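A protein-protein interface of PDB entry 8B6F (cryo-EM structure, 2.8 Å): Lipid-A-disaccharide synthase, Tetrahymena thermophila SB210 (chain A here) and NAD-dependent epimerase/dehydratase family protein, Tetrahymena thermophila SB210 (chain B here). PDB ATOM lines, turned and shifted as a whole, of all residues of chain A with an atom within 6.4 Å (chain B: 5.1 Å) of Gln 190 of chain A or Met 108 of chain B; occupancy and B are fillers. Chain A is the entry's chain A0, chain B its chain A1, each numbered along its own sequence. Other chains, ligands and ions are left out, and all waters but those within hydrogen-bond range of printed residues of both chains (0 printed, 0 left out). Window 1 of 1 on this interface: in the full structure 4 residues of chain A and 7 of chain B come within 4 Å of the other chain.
Of chain B, only His 100 and Met 108 come within 4 Å of Gln 190 of chain A. Of the printed residues of chain A, Met 108 of chain B touches Phe 189 and Gln 190. Of the printed residues of chain A, Arg 99 of chain B touches Phe 189 (3.5 Å). Printed residues of chain B within 4 Å of Ser 191 of chain A: Met 111 (3.5 Å). Printed residues of chain A within 4 Å of His 100 of chain B: Phe 189 and Gln 190. Of the printed residues of chain A, Met 111 of chain B touches Ser 191. Phe 101 of chain B touches none of the printed residues of chain A.
NH1 of Arg 99 of chain B touches CZ of Phe 189 of chain A (3.5 Å). Phe 189 of chain A touches His 100 of chain B. O of Phe 189 of chain A touches CE of Met 108 of chain B, 3.95 Å away. Ser 191 of chain A touches Met 111 of chain B (OG to CE, 3.5 Å).
Of the 13 printed residues of chain B, 4 touch a printed residue of chain A. Of the 6 printed residues of chain A, 3 touch a printed residue of chain B.
The backbone carbonyl oxygen of Gln 190 of chain A lies close to the side-chain sulfur of Met 108 of chain B (3.6 Å). The backbone carbonyl oxygen (O) of His 100 of chain B sits at hydrogen-bond distance from the side-chain amide nitrogen (NE2) of Gln 190 of chain A (3.2 Å).
N of Ser 191 of chain A lies within hydrogen-bond range of OD1 of Asn 188 of chain A (2.9 Å). The side-chain amide oxygen (OD1) of Asn 188 of chain A lies close to the backbone NH (N) of Gln 190 of chain A (3.5 Å). SD of Met 111 of chain B sits close to OD1 of Asn 107 of chain B, 3.6 Å away.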
ATOM      1  N   ARG A 168      -8.071  -0.756   3.072  1.00  0.00           N
ATOM      2  CA  ARG A 168      -7.711   0.153   4.148  1.00  0.00           C
ATOM      3  C   ARG A 168      -7.501  -0.631   5.437  1.00  0.00           C
ATOM      4  O   ARG A 168      -7.994  -1.751   5.595  1.00  0.00           O
ATOM      5  CB  ARG A 168      -8.795   1.220   4.357  1.00  0.00           C
ATOM      6  CG  ARG A 168      -9.125   2.034   3.110  1.00  0.00           C
ATOM      7  CD  ARG A 168      -8.263   3.280   2.998  1.00  0.00           C
ATOM      8  NE  ARG A 168      -8.635   4.287   3.985  1.00  0.00           N
ATOM      9  CZ  ARG A 168      -8.157   5.524   4.013  1.00  0.00           C
ATOM     10  NH1 ARG A 168      -7.283   5.947   3.115  1.00  0.00           N
ATOM     11  NH2 ARG A 168      -8.563   6.356   4.967  1.00  0.00           N
ATOM     12  N   ASN A 188       1.519   2.614  -0.424  1.00  0.00           N
ATOM     13  CA  ASN A 188       0.924   3.706   0.334  1.00  0.00           C
ATOM     14  C   ASN A 188       1.972   4.236   1.302  1.00  0.00           C
ATOM     15  O   ASN A 188       3.014   3.615   1.520  1.00  0.00           O
ATOM     16  CB  ASN A 188      -0.338   3.257   1.075  1.00  0.00           C
ATOM     17  CG  ASN A 188      -0.105   2.041   1.947  1.00  0.00           C
ATOM     18  OD1 ASN A 188       1.014   1.778   2.382  1.00  0.00           O
ATOM     19  ND2 ASN A 188      -1.166   1.286   2.203  1.00  0.00           N
ATOM     20  N   PHE A 189       1.681   5.404   1.877  1.00  0.00           N
ATOM     21  CA  PHE A 189       2.607   6.011   2.824  1.00  0.00           C
ATOM     22  C   PHE A 189       2.600   5.302   4.171  1.00  0.00           C
ATOM     23  O   PHE A 189       3.551   5.457   4.942  1.00  0.00           O
ATOM     24  CB  PHE A 189       2.278   7.492   3.009  1.00  0.00           C
ATOM     25  CG  PHE A 189       2.578   8.332   1.801  1.00  0.00           C
ATOM     26  CD1 PHE A 189       3.854   8.824   1.585  1.00  0.00           C
ATOM     27  CD2 PHE A 189       1.585   8.632   0.886  1.00  0.00           C
ATOM     28  CE1 PHE A 189       4.137   9.596   0.476  1.00  0.00           C
ATOM     29  CE2 PHE A 189       1.860   9.405  -0.228  1.00  0.00           C
ATOM     30  CZ  PHE A 189       3.137   9.889  -0.432  1.00  0.00           C
ATOM     31  N   GLN A 190       1.553   4.530   4.473  1.00  0.00           N
ATOM     32  CA  GLN A 190       1.520   3.773   5.717  1.00  0.00           C
ATOM     33  C   GLN A 190       2.429   2.553   5.693  1.00  0.00           C
ATOM     34  O   GLN A 190       2.673   1.969   6.753  1.00  0.00           O
ATOM     35  CB  GLN A 190       0.092   3.324   6.035  1.00  0.00           C
ATOM     36  CG  GLN A 190      -0.857   4.451   6.412  1.00  0.00           C
ATOM     37  CD  GLN A 190      -1.486   5.115   5.209  1.00  0.00           C
ATOM     38  OE1 GLN A 190      -1.096   4.863   4.069  1.00  0.00           O
ATOM     39  NE2 GLN A 190      -2.473   5.967   5.454  1.00  0.00           N
ATOM     40  N   SER A 191       2.931   2.153   4.526  1.00  0.00           N
ATOM     41  CA  SER A 191       3.722   0.930   4.401  1.00  0.00           C
ATOM     42  C   SER A 191       2.934  -0.267   4.919  1.00  0.00           C
ATOM     43  O   SER A 191       3.490  -1.190   5.518  1.00  0.00           O
ATOM     44  CB  SER A 191       5.059   1.059   5.134  1.00  0.00           C
ATOM     45  OG  SER A 191       5.825   2.132   4.615  1.00  0.00           O
ATOM     46  N   PHE A 192       1.628  -0.252   4.680  1.00  0.00           N
ATOM     47  CA  PHE A 192       0.715  -1.267   5.179  1.00  0.00           C
ATOM     48  C   PHE A 192       0.225  -2.122   4.022  1.00  0.00           C
ATOM     49  O   PHE A 192      -0.239  -1.592   3.008  1.00  0.00           O
ATOM     50  CB  PHE A 192      -0.469  -0.619   5.899  1.00  0.00           C
ATOM     51  CG  PHE A 192      -1.607  -1.560   6.167  1.00  0.00           C
ATOM     52  CD1 PHE A 192      -1.549  -2.453   7.223  1.00  0.00           C
ATOM     53  CD2 PHE A 192      -2.740  -1.537   5.373  1.00  0.00           C
ATOM     54  CE1 PHE A 192      -2.597  -3.316   7.476  1.00  0.00           C
ATOM     55  CE2 PHE A 192      -3.791  -2.397   5.620  1.00  0.00           C
ATOM     56  CZ  PHE A 192      -3.720  -3.288   6.674  1.00  0.00           C
ATOM     57  N   MET B  98       6.324  12.711   8.144  1.00  0.00           N
ATOM     58  CA  MET B  98       5.707  11.413   7.885  1.00  0.00           C
ATOM     59  C   MET B  98       4.199  11.627   7.790  1.00  0.00           C
ATOM     60  O   MET B  98       3.516  11.769   8.806  1.00  0.00           O
ATOM     61  CB  MET B  98       6.077  10.414   8.976  1.00  0.00           C
ATOM     62  CG  MET B  98       5.423   9.052   8.824  1.00  0.00           C
ATOM     63  SD  MET B  98       5.862   7.909  10.149  1.00  0.00           S
ATOM     64  CE  MET B  98       7.641   7.836   9.961  1.00  0.00           C
ATOM     65  N   ARG B  99       3.689  11.637   6.563  1.00  0.00           N
ATOM     66  CA  ARG B  99       2.296  11.943   6.289  1.00  0.00           C
ATOM     67  C   ARG B  99       1.426  10.698   6.426  1.00  0.00           C
ATOM     68  O   ARG B  99       1.908   9.565   6.463  1.00  0.00           O
ATOM     69  CB  ARG B  99       2.149  12.532   4.888  1.00  0.00           C
ATOM     70  CG  ARG B  99       2.288  11.504   3.775  1.00  0.00           C
ATOM     71  CD  ARG B  99       2.404  12.163   2.414  1.00  0.00           C
ATOM     72  NE  ARG B  99       3.706  12.789   2.221  1.00  0.00           N
ATOM     73  CZ  ARG B  99       4.108  13.346   1.088  1.00  0.00           C
ATOM     74  NH1 ARG B  99       3.331  13.377   0.019  1.00  0.00           N
ATOM     75  NH2 ARG B  99       5.322  13.886   1.026  1.00  0.00           N
ATOM     76  N   HIS B 100       0.112  10.928   6.493  1.00  0.00           N
ATOM     77  CA  HIS B 100      -0.874   9.849   6.534  1.00  0.00           C
ATOM     78  C   HIS B 100      -0.589   8.881   7.677  1.00  0.00           C
ATOM     79  O   HIS B 100      -0.728   7.665   7.536  1.00  0.00           O
ATOM     80  CB  HIS B 100      -0.924   9.105   5.199  1.00  0.00           C
ATOM     81  CG  HIS B 100      -1.294   9.977   4.039  1.00  0.00           C
ATOM     82  ND1 HIS B 100      -1.312   9.518   2.740  1.00  0.00           N
ATOM     83  CD2 HIS B 100      -1.659  11.279   3.982  1.00  0.00           C
ATOM     84  CE1 HIS B 100      -1.674  10.499   1.934  1.00  0.00           C
ATOM     85  NE2 HIS B 100      -1.889  11.579   2.662  1.00  0.00           N
ATOM     86  N   PHE B 101      -0.181   9.422   8.821  1.00  0.00           N
ATOM     87  CA  PHE B 101       0.110   8.582   9.971  1.00  0.00           C
ATOM     88  C   PHE B 101      -1.165   7.933  10.491  1.00  0.00           C
ATOM     89  O   PHE B 101      -2.215   8.574  10.586  1.00  0.00           O
ATOM     90  CB  PHE B 101       0.774   9.398  11.077  1.00  0.00           C
ATOM     91  CG  PHE B 101       1.258   8.567  12.229  1.00  0.00           C
ATOM     92  CD1 PHE B 101       0.417   8.256  13.282  1.00  0.00           C
ATOM     93  CD2 PHE B 101       2.557   8.093  12.254  1.00  0.00           C
ATOM     94  CE1 PHE B 101       0.865   7.490  14.339  1.00  0.00           C
ATOM     95  CE2 PHE B 101       3.009   7.326  13.308  1.00  0.00           C
ATOM     96  CZ  PHE B 101       2.163   7.025  14.351  1.00  0.00           C
ATOM     97  N   ASN B 102      -1.068   6.649  10.823  1.00  0.00           N
ATOM     98  CA  ASN B 102      -2.172   5.896  11.399  1.00  0.00           C
ATOM     99  C   ASN B 102      -1.931   5.759  12.896  1.00  0.00           C
ATOM    100  O   ASN B 102      -0.910   5.202  13.314  1.00  0.00           O
ATOM    101  CB  ASN B 102      -2.288   4.523  10.739  1.00  0.00           C
ATOM    102  CG  ASN B 102      -3.596   3.838  11.051  1.00  0.00           C
ATOM    103  OD1 ASN B 102      -4.587   4.487  11.379  1.00  0.00           O
ATOM    104  ND2 ASN B 102      -3.609   2.515  10.950  1.00  0.00           N
ATOM    105  N   ASP B 105      -2.170   1.868  14.726  1.00  0.00           N
ATOM    106  CA  ASP B 105      -1.315   0.782  14.262  1.00  0.00           C
ATOM    107  C   ASP B 105       0.025   0.869  14.977  1.00  0.00           C
ATOM    108  O   ASP B 105       0.690   1.909  14.932  1.00  0.00           O
ATOM    109  CB  ASP B 105      -1.120   0.854  12.746  1.00  0.00           C
ATOM    110  CG  ASP B 105      -0.357  -0.339  12.197  1.00  0.00           C
ATOM    111  OD1 ASP B 105      -0.006  -1.240  12.988  1.00  0.00           O
ATOM    112  OD2 ASP B 105      -0.111  -0.377  10.973  1.00  0.00           O
ATOM    113  N   ASP B 106       0.419  -0.226  15.633  1.00  0.00           N
ATOM    114  CA  ASP B 106       1.684  -0.241  16.361  1.00  0.00           C
ATOM    115  C   ASP B 106       2.877  -0.201  15.418  1.00  0.00           C
ATOM    116  O   ASP B 106       3.918   0.372  15.760  1.00  0.00           O
ATOM    117  CB  ASP B 106       1.766  -1.478  17.252  1.00  0.00           C
ATOM    118  CG  ASP B 106       0.651  -1.535  18.273  1.00  0.00           C
ATOM    119  OD1 ASP B 106       0.209  -0.460  18.731  1.00  0.00           O
ATOM    120  OD2 ASP B 106       0.215  -2.654  18.618  1.00  0.00           O
ATOM    121  N   ASN B 107       2.749  -0.798  14.232  1.00  0.00           N
ATOM    122  CA  ASN B 107       3.849  -0.772  13.275  1.00  0.00           C
ATOM    123  C   ASN B 107       4.184   0.657  12.870  1.00  0.00           C
ATOM    124  O   ASN B 107       5.353   0.990  12.648  1.00  0.00           O
ATOM    125  CB  ASN B 107       3.494  -1.611  12.049  1.00  0.00           C
ATOM    126  CG  ASN B 107       4.586  -1.602  11.002  1.00  0.00           C
ATOM    127  OD1 ASN B 107       5.746  -1.319  11.301  1.00  0.00           O
ATOM    128  ND2 ASN B 107       4.221  -1.914   9.765  1.00  0.00           N
ATOM    129  N   MET B 108       3.170   1.515  12.768  1.00  0.00           N
ATOM    130  CA  MET B 108       3.415   2.907  12.415  1.00  0.00           C
ATOM    131  C   MET B 108       4.271   3.590  13.476  1.00  0.00           C
ATOM    132  O   MET B 108       5.218   4.314  13.153  1.00  0.00           O
ATOM    133  CB  MET B 108       2.086   3.637  12.226  1.00  0.00           C
ATOM    134  CG  MET B 108       2.176   4.796  11.255  1.00  0.00           C
ATOM    135  SD  MET B 108       2.240   4.256   9.538  1.00  0.00           S
ATOM    136  CE  MET B 108       2.419   5.830   8.711  1.00  0.00           C
ATOM    137  N   TYR B 109       3.942   3.376  14.752  1.00  0.00           N
ATOM    138  CA  TYR B 109       4.748   3.947  15.826  1.00  0.00           C
ATOM    139  C   TYR B 109       6.162   3.379  15.820  1.00  0.00           C
ATOM    140  O   TYR B 109       7.135   4.115  16.019  1.00  0.00           O
ATOM    141  CB  TYR B 109       4.085   3.695  17.179  1.00  0.00           C
ATOM    142  CG  TYR B 109       2.730   4.337  17.332  1.00  0.00           C
ATOM    143  CD1 TYR B 109       2.615   5.688  17.632  1.00  0.00           C
ATOM    144  CD2 TYR B 109       1.567   3.594  17.200  1.00  0.00           C
ATOM    145  CE1 TYR B 109       1.383   6.284  17.779  1.00  0.00           C
ATOM    146  CE2 TYR B 109       0.326   4.181  17.347  1.00  0.00           C
ATOM    147  CZ  TYR B 109       0.242   5.527  17.640  1.00  0.00           C
ATOM    148  OH  TYR B 109      -0.987   6.120  17.789  1.00  0.00           O
ATOM    149  N   ASP B 110       6.296   2.072  15.592  1.00  0.00           N
ATOM    150  CA  ASP B 110       7.620   1.462  15.552  1.00  0.00           C
ATOM    151  C   ASP B 110       8.474   2.093  14.461  1.00  0.00           C
ATOM    152  O   ASP B 110       9.645   2.421  14.683  1.00  0.00           O
ATOM    153  CB  ASP B 110       7.495  -0.045  15.333  1.00  0.00           C
ATOM    154  CG  ASP B 110       6.862  -0.753  16.512  1.00  0.00           C
ATOM    155  OD1 ASP B 110       6.541  -0.073  17.508  1.00  0.00           O
ATOM    156  OD2 ASP B 110       6.689  -1.987  16.444  1.00  0.00           O
ATOM    157  N   MET B 111       7.899   2.277  13.273  1.00  0.00           N
ATOM    158  CA  MET B 111       8.628   2.931  12.193  1.00  0.00           C
ATOM    159  C   MET B 111       8.978   4.366  12.559  1.00  0.00           C
ATOM    160  O   MET B 111      10.086   4.835  12.276  1.00  0.00           O
ATOM    161  CB  MET B 111       7.797   2.900  10.912  1.00  0.00           C
ATOM    162  CG  MET B 111       7.538   1.503  10.373  1.00  0.00           C
ATOM    163  SD  MET B 111       6.274   1.476   9.086  1.00  0.00           S
ATOM    164  CE  MET B 111       6.938   2.664   7.922  1.00  0.00           C
ATOM    165  N   ALA B 112       8.046   5.083  13.190  1.00  0.00           N
ATOM    166  CA  ALA B 112       8.282   6.485  13.511  1.00  0.00           C
ATOM    167  C   ALA B 112       9.439   6.653  14.490  1.00  0.00           C
ATOM    168  O   ALA B 112      10.256   7.568  14.338  1.00  0.00           O
ATOM    169  CB  ALA B 112       7.009   7.111  14.076  1.00  0.00           C
